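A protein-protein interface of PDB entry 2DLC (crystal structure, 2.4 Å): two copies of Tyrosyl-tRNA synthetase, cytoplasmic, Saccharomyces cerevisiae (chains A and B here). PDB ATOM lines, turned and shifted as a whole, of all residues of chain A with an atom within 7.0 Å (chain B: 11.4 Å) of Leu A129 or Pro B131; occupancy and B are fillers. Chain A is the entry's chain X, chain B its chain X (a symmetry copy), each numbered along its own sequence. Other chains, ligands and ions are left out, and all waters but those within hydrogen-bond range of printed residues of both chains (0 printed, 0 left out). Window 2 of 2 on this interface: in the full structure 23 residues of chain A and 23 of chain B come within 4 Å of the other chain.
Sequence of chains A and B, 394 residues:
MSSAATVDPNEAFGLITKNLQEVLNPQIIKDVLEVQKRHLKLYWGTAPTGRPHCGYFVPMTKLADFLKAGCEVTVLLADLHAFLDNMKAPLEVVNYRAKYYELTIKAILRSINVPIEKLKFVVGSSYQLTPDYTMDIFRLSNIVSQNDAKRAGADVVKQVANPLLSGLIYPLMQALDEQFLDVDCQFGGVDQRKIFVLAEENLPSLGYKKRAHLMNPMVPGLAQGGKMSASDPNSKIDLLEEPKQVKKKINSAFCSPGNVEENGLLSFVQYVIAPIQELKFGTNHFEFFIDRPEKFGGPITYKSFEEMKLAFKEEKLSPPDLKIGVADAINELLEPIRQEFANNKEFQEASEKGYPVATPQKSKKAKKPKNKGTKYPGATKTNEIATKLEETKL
Pro B131 touches Leu A129. Leu A129 touches Met B135. Phe B138 touches Leu A129 (CE1 to CD2, 3.7 Å). Leu B129 touches Pro A131. SD of Met A173 touches CE2 of Phe B138, 3.6 Å away.
The backbone carbonyl oxygen of Thr A130 sits at hydrogen-bond distance from the side-chain hydroxyl of Thr A134 (3.2 Å). OH of Tyr A133 sits at hydrogen-bond distance from O of Met A173 (2.8 Å). The side-chain hydroxyl (OG1) of Thr B134 lies within hydrogen-bond range of the backbone carbonyl oxygen (O) of Thr B130, 3.2 Å away. The backbone carbonyl oxygen of Phe B138 lies within hydrogen-bond range of the side-chain hydroxyl of Ser B141 (2.8 Å).
Of the 13 printed residues of chain A, 4 touch a printed residue of chain B. Hydrophobic or aromatic side chains of chain A within 4 Å of the printed part of chain B: Leu A129, Pro A131 and Met A173. Among the printed residues, 6 pairs touch across the chains. Among the printed residues, no Asp or Glu carboxylate lies within 4 Å of a Lys or Arg side-chain nitrogen of the other chain.
Leu A129 touches Pro B131, and with the chains exchanged Pro A131 touches Leu B129. Thr A134 touches its own counterpart, Thr B134. Positions printed for both chains: 80, 124, 125, 126, 127, 128, 129, 130, 131, 132, 133 and 134. Of the 6 pairs that touch across the chains among the printed residues, 3 have their exchanged pair printed and touching as well.
OG1 of Thr A134 sits at hydrogen-bond distance from OG1 of Thr B134, at 2.7 Å.
Of chain B, only Pro B131 (3.3 Å), Met B135 (3.9 Å) and Phe B138 (3.7 Å) come within 4 Å of Leu A129. Printed residues of chain A within 4 Å of Pro B131: Leu A129 (3.3 Å). Gln A128 touches none of the printed residues of chain B. No residue of chain B comes within 4 Å of Thr A130. Printed residues of chain B within 4 Å of Met A173: Phe B138 (3.6 Å). Printed residues of chain A within 4 Å of Met B135: Leu A129 (3.9 Å). Of the printed residues of chain A, Thr B134 touches Thr A134. Ser B126 touches none of the printed residues of chain A. Gly A124 touches none of the printed residues of chain B. The nearest residue of chain B that does not touch Leu A129 is Thr B134 (4.2 Å). The nearest residue of chain A that does not touch Pro B131 is Thr A130 (5.1 Å).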
ATOM      1  N   LEU A  80      -4.306 -10.439  -2.777  1.00  0.00           N
ATOM      2  CA  LEU A  80      -4.946 -11.726  -2.502  1.00  0.00           C
ATOM      3  C   LEU A  80      -4.809 -12.688  -3.685  1.00  0.00           C
ATOM      4  O   LEU A  80      -4.561 -13.881  -3.495  1.00  0.00           O
ATOM      5  CB  LEU A  80      -6.415 -11.526  -2.131  1.00  0.00           C
ATOM      6  CG  LEU A  80      -6.789 -11.548  -0.644  1.00  0.00           C
ATOM      7  CD1 LEU A  80      -5.629 -11.174   0.282  1.00  0.00           C
ATOM      8  CD2 LEU A  80      -7.997 -10.664  -0.388  1.00  0.00           C
ATOM      9  N   GLY A 124      -6.374  -5.001  -3.344  1.00  0.00           N
ATOM     10  CA  GLY A 124      -7.480  -5.933  -3.463  1.00  0.00           C
ATOM     11  C   GLY A 124      -8.118  -6.373  -2.157  1.00  0.00           C
ATOM     12  O   GLY A 124      -9.342  -6.447  -2.074  1.00  0.00           O
ATOM     13  N   SER A 125      -7.303  -6.652  -1.139  1.00  0.00           N
ATOM     14  CA  SER A 125      -7.816  -7.108   0.157  1.00  0.00           C
ATOM     15  C   SER A 125      -8.681  -6.084   0.901  1.00  0.00           C
ATOM     16  O   SER A 125      -9.343  -6.429   1.884  1.00  0.00           O
ATOM     17  CB  SER A 125      -6.678  -7.597   1.057  1.00  0.00           C
ATOM     18  OG  SER A 125      -5.774  -6.557   1.370  1.00  0.00           O
ATOM     19  N   SER A 126      -8.683  -4.838   0.428  1.00  0.00           N
ATOM     20  CA  SER A 126      -9.440  -3.763   1.080  1.00  0.00           C
ATOM     21  C   SER A 126     -10.946  -3.858   0.823  1.00  0.00           C
ATOM     22  O   SER A 126     -11.732  -3.174   1.487  1.00  0.00           O
ATOM     23  CB  SER A 126      -8.921  -2.391   0.639  1.00  0.00           C
ATOM     24  OG  SER A 126      -9.348  -2.088  -0.678  1.00  0.00           O
ATOM     25  N   TYR A 127     -11.339  -4.682  -0.149  1.00  0.00           N
ATOM     26  CA  TYR A 127     -12.757  -4.952  -0.404  1.00  0.00           C
ATOM     27  C   TYR A 127     -13.051  -6.433  -0.649  1.00  0.00           C
ATOM     28  O   TYR A 127     -14.198  -6.866  -0.538  1.00  0.00           O
ATOM     29  CB  TYR A 127     -13.274  -4.116  -1.576  1.00  0.00           C
ATOM     30  CG  TYR A 127     -12.649  -4.483  -2.907  1.00  0.00           C
ATOM     31  CD1 TYR A 127     -11.521  -3.808  -3.379  1.00  0.00           C
ATOM     32  CD2 TYR A 127     -13.186  -5.504  -3.690  1.00  0.00           C
ATOM     33  CE1 TYR A 127     -10.942  -4.146  -4.600  1.00  0.00           C
ATOM     34  CE2 TYR A 127     -12.619  -5.846  -4.910  1.00  0.00           C
ATOM     35  CZ  TYR A 127     -11.501  -5.159  -5.358  1.00  0.00           C
ATOM     36  OH  TYR A 127     -10.938  -5.499  -6.558  1.00  0.00           O
ATOM     37  N   GLN A 128     -12.017  -7.204  -0.974  1.00  0.00           N
ATOM     38  CA  GLN A 128     -12.191  -8.614  -1.308  1.00  0.00           C
ATOM     39  C   GLN A 128     -12.506  -9.519  -0.109  1.00  0.00           C
ATOM     40  O   GLN A 128     -12.855 -10.677  -0.294  1.00  0.00           O
ATOM     41  CB  GLN A 128     -10.978  -9.142  -2.081  1.00  0.00           C
ATOM     42  CG  GLN A 128     -10.865  -8.584  -3.503  1.00  0.00           C
ATOM     43  CD  GLN A 128      -9.557  -8.938  -4.187  1.00  0.00           C
ATOM     44  OE1 GLN A 128      -8.555  -9.237  -3.527  1.00  0.00           O
ATOM     45  NE2 GLN A 128      -9.559  -8.899  -5.512  1.00  0.00           N
ATOM     46  N   LEU A 129     -12.394  -8.986   1.107  1.00  0.00           N
ATOM     47  CA  LEU A 129     -12.745  -9.732   2.317  1.00  0.00           C
ATOM     48  C   LEU A 129     -14.057  -9.275   2.971  1.00  0.00           C
ATOM     49  O   LEU A 129     -14.439  -9.802   4.019  1.00  0.00           O
ATOM     50  CB  LEU A 129     -11.599  -9.703   3.345  1.00  0.00           C
ATOM     51  CG  LEU A 129     -10.239 -10.254   2.897  1.00  0.00           C
ATOM     52  CD1 LEU A 129      -9.141  -9.858   3.888  1.00  0.00           C
ATOM     53  CD2 LEU A 129     -10.282 -11.776   2.690  1.00  0.00           C
ATOM     54  N   THR A 130     -14.744  -8.317   2.353  1.00  0.00           N
ATOM     55  CA  THR A 130     -16.065  -7.888   2.813  1.00  0.00           C
ATOM     56  C   THR A 130     -17.141  -8.952   2.518  1.00  0.00           C
ATOM     57  O   THR A 130     -16.982  -9.756   1.596  1.00  0.00           O
ATOM     58  CB  THR A 130     -16.459  -6.515   2.186  1.00  0.00           C
ATOM     59  OG1 THR A 130     -16.527  -6.627   0.759  1.00  0.00           O
ATOM     60  CG2 THR A 130     -15.376  -5.470   2.418  1.00  0.00           C
ATOM     61  N   PRO A 131     -18.223  -8.965   3.304  1.00  0.00           N
ATOM     62  CA  PRO A 131     -19.317  -9.935   3.117  1.00  0.00           C
ATOM     63  C   PRO A 131     -19.999  -9.923   1.736  1.00  0.00           C
ATOM     64  O   PRO A 131     -20.313 -10.996   1.210  1.00  0.00           O
ATOM     65  CB  PRO A 131     -20.316  -9.553   4.225  1.00  0.00           C
ATOM     66  CG  PRO A 131     -19.488  -8.851   5.264  1.00  0.00           C
ATOM     67  CD  PRO A 131     -18.460  -8.088   4.468  1.00  0.00           C
ATOM     68  N   ASP A 132     -20.225  -8.741   1.163  1.00  0.00           N
ATOM     69  CA  ASP A 132     -20.853  -8.620  -0.153  1.00  0.00           C
ATOM     70  C   ASP A 132     -20.025  -9.324  -1.231  1.00  0.00           C
ATOM     71  O   ASP A 132     -20.573 -10.020  -2.093  1.00  0.00           O
ATOM     72  CB  ASP A 132     -21.067  -7.147  -0.533  1.00  0.00           C
ATOM     73  CG  ASP A 132     -22.196  -6.480   0.254  1.00  0.00           C
ATOM     74  OD1 ASP A 132     -23.056  -7.180   0.831  1.00  0.00           O
ATOM     75  OD2 ASP A 132     -22.307  -5.237   0.339  1.00  0.00           O
ATOM     76  N   TYR A 133     -18.707  -9.136  -1.175  1.00  0.00           N
ATOM     77  CA  TYR A 133     -17.776  -9.812  -2.085  1.00  0.00           C
ATOM     78  C   TYR A 133     -17.802 -11.336  -1.911  1.00  0.00           C
ATOM     79  O   TYR A 133     -17.924 -12.070  -2.893  1.00  0.00           O
ATOM     80  CB  TYR A 133     -16.353  -9.269  -1.901  1.00  0.00           C
ATOM     81  CG  TYR A 133     -15.417  -9.569  -3.045  1.00  0.00           C
ATOM     82  CD1 TYR A 133     -14.622 -10.722  -3.044  1.00  0.00           C
ATOM     83  CD2 TYR A 133     -15.313  -8.698  -4.132  1.00  0.00           C
ATOM     84  CE1 TYR A 133     -13.750 -10.999  -4.101  1.00  0.00           C
ATOM     85  CE2 TYR A 133     -14.450  -8.969  -5.191  1.00  0.00           C
ATOM     86  CZ  TYR A 133     -13.673 -10.117  -5.167  1.00  0.00           C
ATOM     87  OH  TYR A 133     -12.818 -10.380  -6.215  1.00  0.00           O
ATOM     88  N   THR A 134     -17.707 -11.798  -0.664  1.00  0.00           N
ATOM     89  CA  THR A 134     -17.730 -13.234  -0.365  1.00  0.00           C
ATOM     90  C   THR A 134     -19.011 -13.877  -0.875  1.00  0.00           C
ATOM     91  O   THR A 134     -18.966 -14.924  -1.523  1.00  0.00           O
ATOM     92  CB  THR A 134     -17.562 -13.486   1.147  1.00  0.00           C
ATOM     93  OG1 THR A 134     -16.360 -12.860   1.592  1.00  0.00           O
ATOM     94  CG2 THR A 134     -17.289 -14.952   1.422  1.00  0.00           C
ATOM     95  N   MET A 173     -12.801 -14.206  -8.901  1.00  0.00           N
ATOM     96  CA  MET A 173     -12.478 -12.976  -8.199  1.00  0.00           C
ATOM     97  C   MET A 173     -12.052 -11.847  -9.147  1.00  0.00           C
ATOM     98  O   MET A 173     -12.427 -10.686  -8.935  1.00  0.00           O
ATOM     99  CB  MET A 173     -11.408 -13.230  -7.132  1.00  0.00           C
ATOM    100  CG  MET A 173     -11.925 -14.037  -5.954  1.00  0.00           C
ATOM    101  SD  MET A 173     -10.712 -14.317  -4.666  1.00  0.00           S
ATOM    102  CE  MET A 173     -10.185 -12.678  -4.243  1.00  0.00           C
ATOM    103  N   LEU B  80     -25.849 -21.296   3.910  1.00  0.00           N
ATOM    104  CA  LEU B  80     -24.960 -21.032   2.779  1.00  0.00           C
ATOM    105  C   LEU B  80     -24.547 -22.325   2.071  1.00  0.00           C
ATOM    106  O   LEU B  80     -24.492 -22.374   0.841  1.00  0.00           O
ATOM    107  CB  LEU B  80     -23.731 -20.245   3.235  1.00  0.00           C
ATOM    108  CG  LEU B  80     -23.721 -18.730   2.999  1.00  0.00           C
ATOM    109  CD1 LEU B  80     -25.121 -18.119   2.898  1.00  0.00           C
ATOM    110  CD2 LEU B  80     -22.899 -18.033   4.068  1.00  0.00           C
ATOM    111  N   GLY B 124     -25.293 -20.529   9.679  1.00  0.00           N
ATOM    112  CA  GLY B 124     -23.977 -20.462   9.073  1.00  0.00           C
ATOM    113  C   GLY B 124     -23.563 -19.103   8.537  1.00  0.00           C
ATOM    114  O   GLY B 124     -22.420 -18.694   8.734  1.00  0.00           O
ATOM    115  N   SER B 125     -24.482 -18.397   7.877  1.00  0.00           N
ATOM    116  CA  SER B 125     -24.178 -17.084   7.300  1.00  0.00           C
ATOM    117  C   SER B 125     -23.828 -15.998   8.324  1.00  0.00           C
ATOM    118  O   SER B 125     -23.343 -14.926   7.950  1.00  0.00           O
ATOM    119  CB  SER B 125     -25.312 -16.609   6.388  1.00  0.00           C
ATOM    120  OG  SER B 125     -26.516 -16.420   7.104  1.00  0.00           O
ATOM    121  N   SER B 126     -24.061 -16.279   9.606  1.00  0.00           N
ATOM    122  CA  SER B 126     -23.804 -15.304  10.671  1.00  0.00           C
ATOM    123  C   SER B 126     -22.313 -15.144  10.982  1.00  0.00           C
ATOM    124  O   SER B 126     -21.924 -14.203  11.681  1.00  0.00           O
ATOM    125  CB  SER B 126     -24.565 -15.682  11.946  1.00  0.00           C
ATOM    126  OG  SER B 126     -23.945 -16.776  12.600  1.00  0.00           O
ATOM    127  N   TYR B 127     -21.493 -16.072  10.487  1.00  0.00           N
ATOM    128  CA  TYR B 127     -20.037 -15.959  10.610  1.00  0.00           C
ATOM    129  C   TYR B 127     -19.296 -16.310   9.319  1.00  0.00           C
ATOM    130  O   TYR B 127     -18.133 -15.946   9.150  1.00  0.00           O
ATOM    131  CB  TYR B 127     -19.514 -16.818  11.763  1.00  0.00           C
ATOM    132  CG  TYR B 127     -19.687 -18.307  11.538  1.00  0.00           C
ATOM    133  CD1 TYR B 127     -20.816 -18.977  12.015  1.00  0.00           C
ATOM    134  CD2 TYR B 127     -18.722 -19.041  10.850  1.00  0.00           C
ATOM    135  CE1 TYR B 127     -20.979 -20.344  11.806  1.00  0.00           C
ATOM    136  CE2 TYR B 127     -18.873 -20.405  10.641  1.00  0.00           C
ATOM    137  CZ  TYR B 127     -20.002 -21.048  11.126  1.00  0.00           C
ATOM    138  OH  TYR B 127     -20.154 -22.391  10.915  1.00  0.00           O
ATOM    139  N   GLN B 128     -19.972 -17.010   8.412  1.00  0.00           N
ATOM    140  CA  GLN B 128     -19.342 -17.470   7.178  1.00  0.00           C
ATOM    141  C   GLN B 128     -19.076 -16.365   6.147  1.00  0.00           C
ATOM    142  O   GLN B 128     -18.386 -16.600   5.164  1.00  0.00           O
ATOM    143  CB  GLN B 128     -20.148 -18.613   6.551  1.00  0.00           C
ATOM    144  CG  GLN B 128     -20.077 -19.922   7.344  1.00  0.00           C
ATOM    145  CD  GLN B 128     -21.041 -20.982   6.843  1.00  0.00           C
ATOM    146  OE1 GLN B 128     -22.045 -20.672   6.192  1.00  0.00           O
ATOM    147  NE2 GLN B 128     -20.742 -22.237   7.148  1.00  0.00           N
ATOM    148  N   LEU B 129     -19.609 -15.167   6.382  1.00  0.00           N
ATOM    149  CA  LEU B 129     -19.356 -14.019   5.509  1.00  0.00           C
ATOM    150  C   LEU B 129     -18.411 -12.973   6.115  1.00  0.00           C
ATOM    151  O   LEU B 129     -18.152 -11.941   5.490  1.00  0.00           O
ATOM    152  CB  LEU B 129     -20.672 -13.355   5.063  1.00  0.00           C
ATOM    153  CG  LEU B 129     -21.683 -14.231   4.314  1.00  0.00           C
ATOM    154  CD1 LEU B 129     -23.047 -13.539   4.234  1.00  0.00           C
ATOM    155  CD2 LEU B 129     -21.174 -14.622   2.917  1.00  0.00           C
ATOM    156  N   THR B 130     -17.892 -13.241   7.312  1.00  0.00           N
ATOM    157  CA  THR B 130     -16.886 -12.379   7.933  1.00  0.00           C
ATOM    158  C   THR B 130     -15.519 -12.506   7.230  1.00  0.00           C
ATOM    159  O   THR B 130     -15.231 -13.536   6.615  1.00  0.00           O
ATOM    160  CB  THR B 130     -16.753 -12.681   9.457  1.00  0.00           C
ATOM    161  OG1 THR B 130     -16.327 -14.035   9.655  1.00  0.00           O
ATOM    162  CG2 THR B 130     -18.106 -12.619  10.154  1.00  0.00           C
ATOM    163  N   PRO B 131     -14.690 -11.461   7.309  1.00  0.00           N
ATOM    164  CA  PRO B 131     -13.357 -11.466   6.678  1.00  0.00           C
ATOM    165  C   PRO B 131     -12.404 -12.590   7.127  1.00  0.00           C
ATOM    166  O   PRO B 131     -11.693 -13.149   6.286  1.00  0.00           O
ATOM    167  CB  PRO B 131     -12.788 -10.084   7.049  1.00  0.00           C
ATOM    168  CG  PRO B 131     -13.996  -9.230   7.314  1.00  0.00           C
ATOM    169  CD  PRO B 131     -14.981 -10.169   7.963  1.00  0.00           C
ATOM    170  N   ASP B 132     -12.388 -12.913   8.420  1.00  0.00           N
ATOM    171  CA  ASP B 132     -11.530 -13.975   8.948  1.00  0.00           C
ATOM    172  C   ASP B 132     -11.858 -15.325   8.304  1.00  0.00           C
ATOM    173  O   ASP B 132     -10.954 -16.088   7.944  1.00  0.00           O
ATOM    174  CB  ASP B 132     -11.650 -14.078  10.476  1.00  0.00           C
ATOM    175  CG  ASP B 132     -10.964 -12.927  11.213  1.00  0.00           C
ATOM    176  OD1 ASP B 132     -10.103 -12.235  10.630  1.00  0.00           O
ATOM    177  OD2 ASP B 132     -11.224 -12.648  12.404  1.00  0.00           O
ATOM    178  N   TYR B 133     -13.152 -15.611   8.166  1.00  0.00           N
ATOM    179  CA  TYR B 133     -13.621 -16.825   7.492  1.00  0.00           C
ATOM    180  C   TYR B 133     -13.216 -16.859   6.013  1.00  0.00           C
ATOM    181  O   TYR B 133     -12.672 -17.858   5.541  1.00  0.00           O
ATOM    182  CB  TYR B 133     -15.141 -16.971   7.641  1.00  0.00           C
ATOM    183  CG  TYR B 133     -15.666 -18.359   7.369  1.00  0.00           C
ATOM    184  CD1 TYR B 133     -16.088 -18.734   6.089  1.00  0.00           C
ATOM    185  CD2 TYR B 133     -15.752 -19.304   8.395  1.00  0.00           C
ATOM    186  CE1 TYR B 133     -16.579 -20.019   5.837  1.00  0.00           C
ATOM    187  CE2 TYR B 133     -16.236 -20.587   8.151  1.00  0.00           C
ATOM    188  CZ  TYR B 133     -16.649 -20.934   6.874  1.00  0.00           C
ATOM    189  OH  TYR B 133     -17.130 -22.203   6.638  1.00  0.00           O
ATOM    190  N   THR B 134     -13.466 -15.762   5.298  1.00  0.00           N
ATOM    191  CA  THR B 134     -13.116 -15.664   3.877  1.00  0.00           C
ATOM    192  C   THR B 134     -11.625 -15.882   3.665  1.00  0.00           C
ATOM    193  O   THR B 134     -11.227 -16.653   2.790  1.00  0.00           O
ATOM    194  CB  THR B 134     -13.554 -14.306   3.292  1.00  0.00           C
ATOM    195  OG1 THR B 134     -14.951 -14.131   3.519  1.00  0.00           O
ATOM    196  CG2 THR B 134     -13.467 -14.318   1.778  1.00  0.00           C
ATOM    197  N   MET B 135     -10.813 -15.203   4.476  1.00  0.00           N
ATOM    198  CA  MET B 135      -9.363 -15.387   4.471  1.00  0.00           C
ATOM    199  C   MET B 135      -8.979 -16.861   4.657  1.00  0.00           C
ATOM    200  O   MET B 135      -8.103 -17.367   3.965  1.00  0.00           O
ATOM    201  CB  MET B 135      -8.725 -14.513   5.559  1.00  0.00           C
ATOM    202  CG  MET B 135      -7.239 -14.252   5.395  1.00  0.00           C
ATOM    203  SD  MET B 135      -6.797 -13.498   3.810  1.00  0.00           S
ATOM    204  CE  MET B 135      -5.475 -14.611   3.339  1.00  0.00           C
ATOM    205  N   ASP B 136      -9.646 -17.546   5.587  1.00  0.00           N
ATOM    206  CA  ASP B 136      -9.400 -18.966   5.808  1.00  0.00           C
ATOM    207  C   ASP B 136      -9.891 -19.867   4.667  1.00  0.00           C
ATOM    208  O   ASP B 136      -9.311 -20.936   4.438  1.00  0.00           O
ATOM    209  CB  ASP B 136      -9.978 -19.422   7.141  1.00  0.00           C
ATOM    210  CG  ASP B 136      -9.072 -19.100   8.311  1.00  0.00           C
ATOM    211  OD1 ASP B 136      -7.921 -18.641   8.103  1.00  0.00           O
ATOM    212  OD2 ASP B 136      -9.438 -19.271   9.490  1.00  0.00           O
ATOM    213  N   ILE B 137     -10.930 -19.447   3.941  1.00  0.00           N
ATOM    214  CA  ILE B 137     -11.301 -20.167   2.715  1.00  0.00           C
ATOM    215  C   ILE B 137     -10.120 -20.115   1.745  1.00  0.00           C
ATOM    216  O   ILE B 137      -9.729 -21.145   1.182  1.00  0.00           O
ATOM    217  CB  ILE B 137     -12.594 -19.619   2.048  1.00  0.00           C
ATOM    218  CG1 ILE B 137     -13.799 -19.743   2.979  1.00  0.00           C
ATOM    219  CG2 ILE B 137     -12.897 -20.365   0.738  1.00  0.00           C
ATOM    220  CD1 ILE B 137     -15.010 -18.944   2.505  1.00  0.00           C
ATOM    221  N   PHE B 138      -9.543 -18.921   1.580  1.00  0.00           N
ATOM    222  CA  PHE B 138      -8.399 -18.725   0.686  1.00  0.00           C
ATOM    223  C   PHE B 138      -7.193 -19.563   1.131  1.00  0.00           C
ATOM    224  O   PHE B 138      -6.556 -20.229   0.313  1.00  0.00           O
ATOM    225  CB  PHE B 138      -8.018 -17.240   0.576  1.00  0.00           C
ATOM    226  CG  PHE B 138      -9.102 -16.356  -0.006  1.00  0.00           C
ATOM    227  CD1 PHE B 138      -9.253 -15.040   0.440  1.00  0.00           C
ATOM    228  CD2 PHE B 138      -9.962 -16.826  -1.006  1.00  0.00           C
ATOM    229  CE1 PHE B 138     -10.240 -14.206  -0.096  1.00  0.00           C
ATOM    230  CE2 PHE B 138     -10.954 -16.001  -1.543  1.00  0.00           C
ATOM    231  CZ  PHE B 138     -11.092 -14.688  -1.087  1.00  0.00           C
ATOM    232  N   ARG B 139      -6.905 -19.547   2.430  1.00  0.00           N
ATOM    233  CA  ARG B 139      -5.800 -20.335   2.981  1.00  0.00           C
ATOM    234  C   ARG B 139      -5.955 -21.837   2.739  1.00  0.00           C
ATOM    235  O   ARG B 139      -5.012 -22.487   2.283  1.00  0.00           O
ATOM    236  CB  ARG B 139      -5.600 -20.044   4.474  1.00  0.00           C
ATOM    237  CG  ARG B 139      -5.110 -18.626   4.759  1.00  0.00           C
ATOM    238  CD  ARG B 139      -4.326 -18.482   6.046  1.00  0.00           C
ATOM    239  NE  ARG B 139      -5.159 -18.756   7.212  1.00  0.00           N
ATOM    240  CZ  ARG B 139      -4.759 -19.428   8.286  1.00  0.00           C
ATOM    241  NH1 ARG B 139      -3.522 -19.902   8.357  1.00  0.00           N
ATOM    242  NH2 ARG B 139      -5.601 -19.617   9.294  1.00  0.00           N
ATOM    243  N   LEU B 140      -7.138 -22.373   3.037  1.00  0.00           N
ATOM    244  CA  LEU B 140      -7.444 -23.779   2.788  1.00  0.00           C
ATOM    245  C   LEU B 140      -7.412 -24.132   1.300  1.00  0.00           C
ATOM    246  O   LEU B 140      -6.920 -25.197   0.932  1.00  0.00           O
ATOM    247  CB  LEU B 140      -8.810 -24.168   3.377  1.00  0.00           C
ATOM    248  CG  LEU B 140      -8.892 -25.252   4.463  1.00  0.00           C
ATOM    249  CD1 LEU B 140     -10.276 -25.877   4.495  1.00  0.00           C
ATOM    250  CD2 LEU B 140      -7.796 -26.338   4.355  1.00  0.00           C
ATOM    251  N   SER B 141      -7.929 -23.239   0.456  1.00  0.00           N
ATOM    252  CA  SER B 141      -7.945 -23.459  -0.997  1.00  0.00           C
ATOM    253  C   SER B 141      -6.528 -23.544  -1.556  1.00  0.00           C
ATOM    254  O   SER B 141      -6.291 -24.104  -2.636  1.00  0.00           O
ATOM    255  CB  SER B 141      -8.736 -22.353  -1.708  1.00  0.00           C
ATOM    256  OG  SER B 141      -7.937 -21.205  -1.935  1.00  0.00           O
ATOM    257  N   LEU B 176     -13.821 -25.707   8.029  1.00  0.00           N
ATOM    258  CA  LEU B 176     -13.514 -24.473   8.746  1.00  0.00           C
ATOM    259  C   LEU B 176     -14.524 -24.207   9.857  1.00  0.00           C
ATOM    260  O   LEU B 176     -14.181 -23.623  10.896  1.00  0.00           O
ATOM    261  CB  LEU B 176     -13.453 -23.286   7.783  1.00  0.00           C
ATOM    262  CG  LEU B 176     -12.286 -23.210   6.793  1.00  0.00           C
ATOM    263  CD1 LEU B 176     -12.467 -22.019   5.844  1.00  0.00           C
ATOM    264  CD2 LEU B 176     -10.940 -23.117   7.500  1.00  0.00           C
ATOM    265  N   PHE B 180     -14.357 -22.332  13.548  1.00  0.00           N
ATOM    266  CA  PHE B 180     -15.128 -21.124  13.814  1.00  0.00           C
ATOM    267  C   PHE B 180     -16.241 -21.331  14.840  1.00  0.00           C
ATOM    268  O   PHE B 180     -16.597 -20.399  15.560  1.00  0.00           O
ATOM    269  CB  PHE B 180     -15.634 -20.499  12.510  1.00  0.00           C
ATOM    270  CG  PHE B 180     -14.602 -19.647  11.825  1.00  0.00           C
ATOM    271  CD1 PHE B 180     -13.547 -20.239  11.128  1.00  0.00           C
ATOM    272  CD2 PHE B 180     -14.662 -18.260  11.904  1.00  0.00           C
ATOM    273  CE1 PHE B 180     -12.578 -19.468  10.505  1.00  0.00           C
ATOM    274  CE2 PHE B 180     -13.693 -17.469  11.282  1.00  0.00           C
ATOM    275  CZ  PHE B 180     -12.647 -18.076  10.580  1.00  0.00           C
ATOM    276  N   LEU B 206      -3.432 -25.100   8.924  1.00  0.00           N
ATOM    277  CA  LEU B 206      -3.855 -23.705   9.073  1.00  0.00           C
ATOM    278  C   LEU B 206      -3.493 -23.104  10.435  1.00  0.00           C
ATOM    279  O   LEU B 206      -3.625 -21.896  10.642  1.00  0.00           O
ATOM    280  CB  LEU B 206      -5.360 -23.589   8.839  1.00  0.00           C
ATOM    281  CG  LEU B 206      -5.906 -23.040   7.511  1.00  0.00           C
ATOM    282  CD1 LEU B 206      -5.088 -23.434   6.291  1.00  0.00           C
ATOM    283  CD2 LEU B 206      -7.335 -23.512   7.350  1.00  0.00           C
ATOM    284  N   TYR B 208      -4.862 -24.629  13.204  1.00  0.00           N
ATOM    285  CA  TYR B 208      -6.005 -25.014  14.030  1.00  0.00           C
ATOM    286  C   TYR B 208      -5.904 -26.464  14.489  1.00  0.00           C
ATOM    287  O   TYR B 208      -5.301 -27.295  13.814  1.00  0.00           O
ATOM    288  CB  TYR B 208      -7.312 -24.790  13.268  1.00  0.00           C
ATOM    289  CG  TYR B 208      -7.491 -23.373  12.756  1.00  0.00           C
ATOM    290  CD1 TYR B 208      -7.132 -22.272  13.540  1.00  0.00           C
ATOM    291  CD2 TYR B 208      -8.018 -23.135  11.487  1.00  0.00           C
ATOM    292  CE1 TYR B 208      -7.292 -20.969  13.068  1.00  0.00           C
ATOM    293  CE2 TYR B 208      -8.185 -21.845  11.009  1.00  0.00           C
ATOM    294  CZ  TYR B 208      -7.819 -20.765  11.803  1.00  0.00           C
ATOM    295  OH  TYR B 208      -7.984 -19.479  11.337  1.00  0.00           O
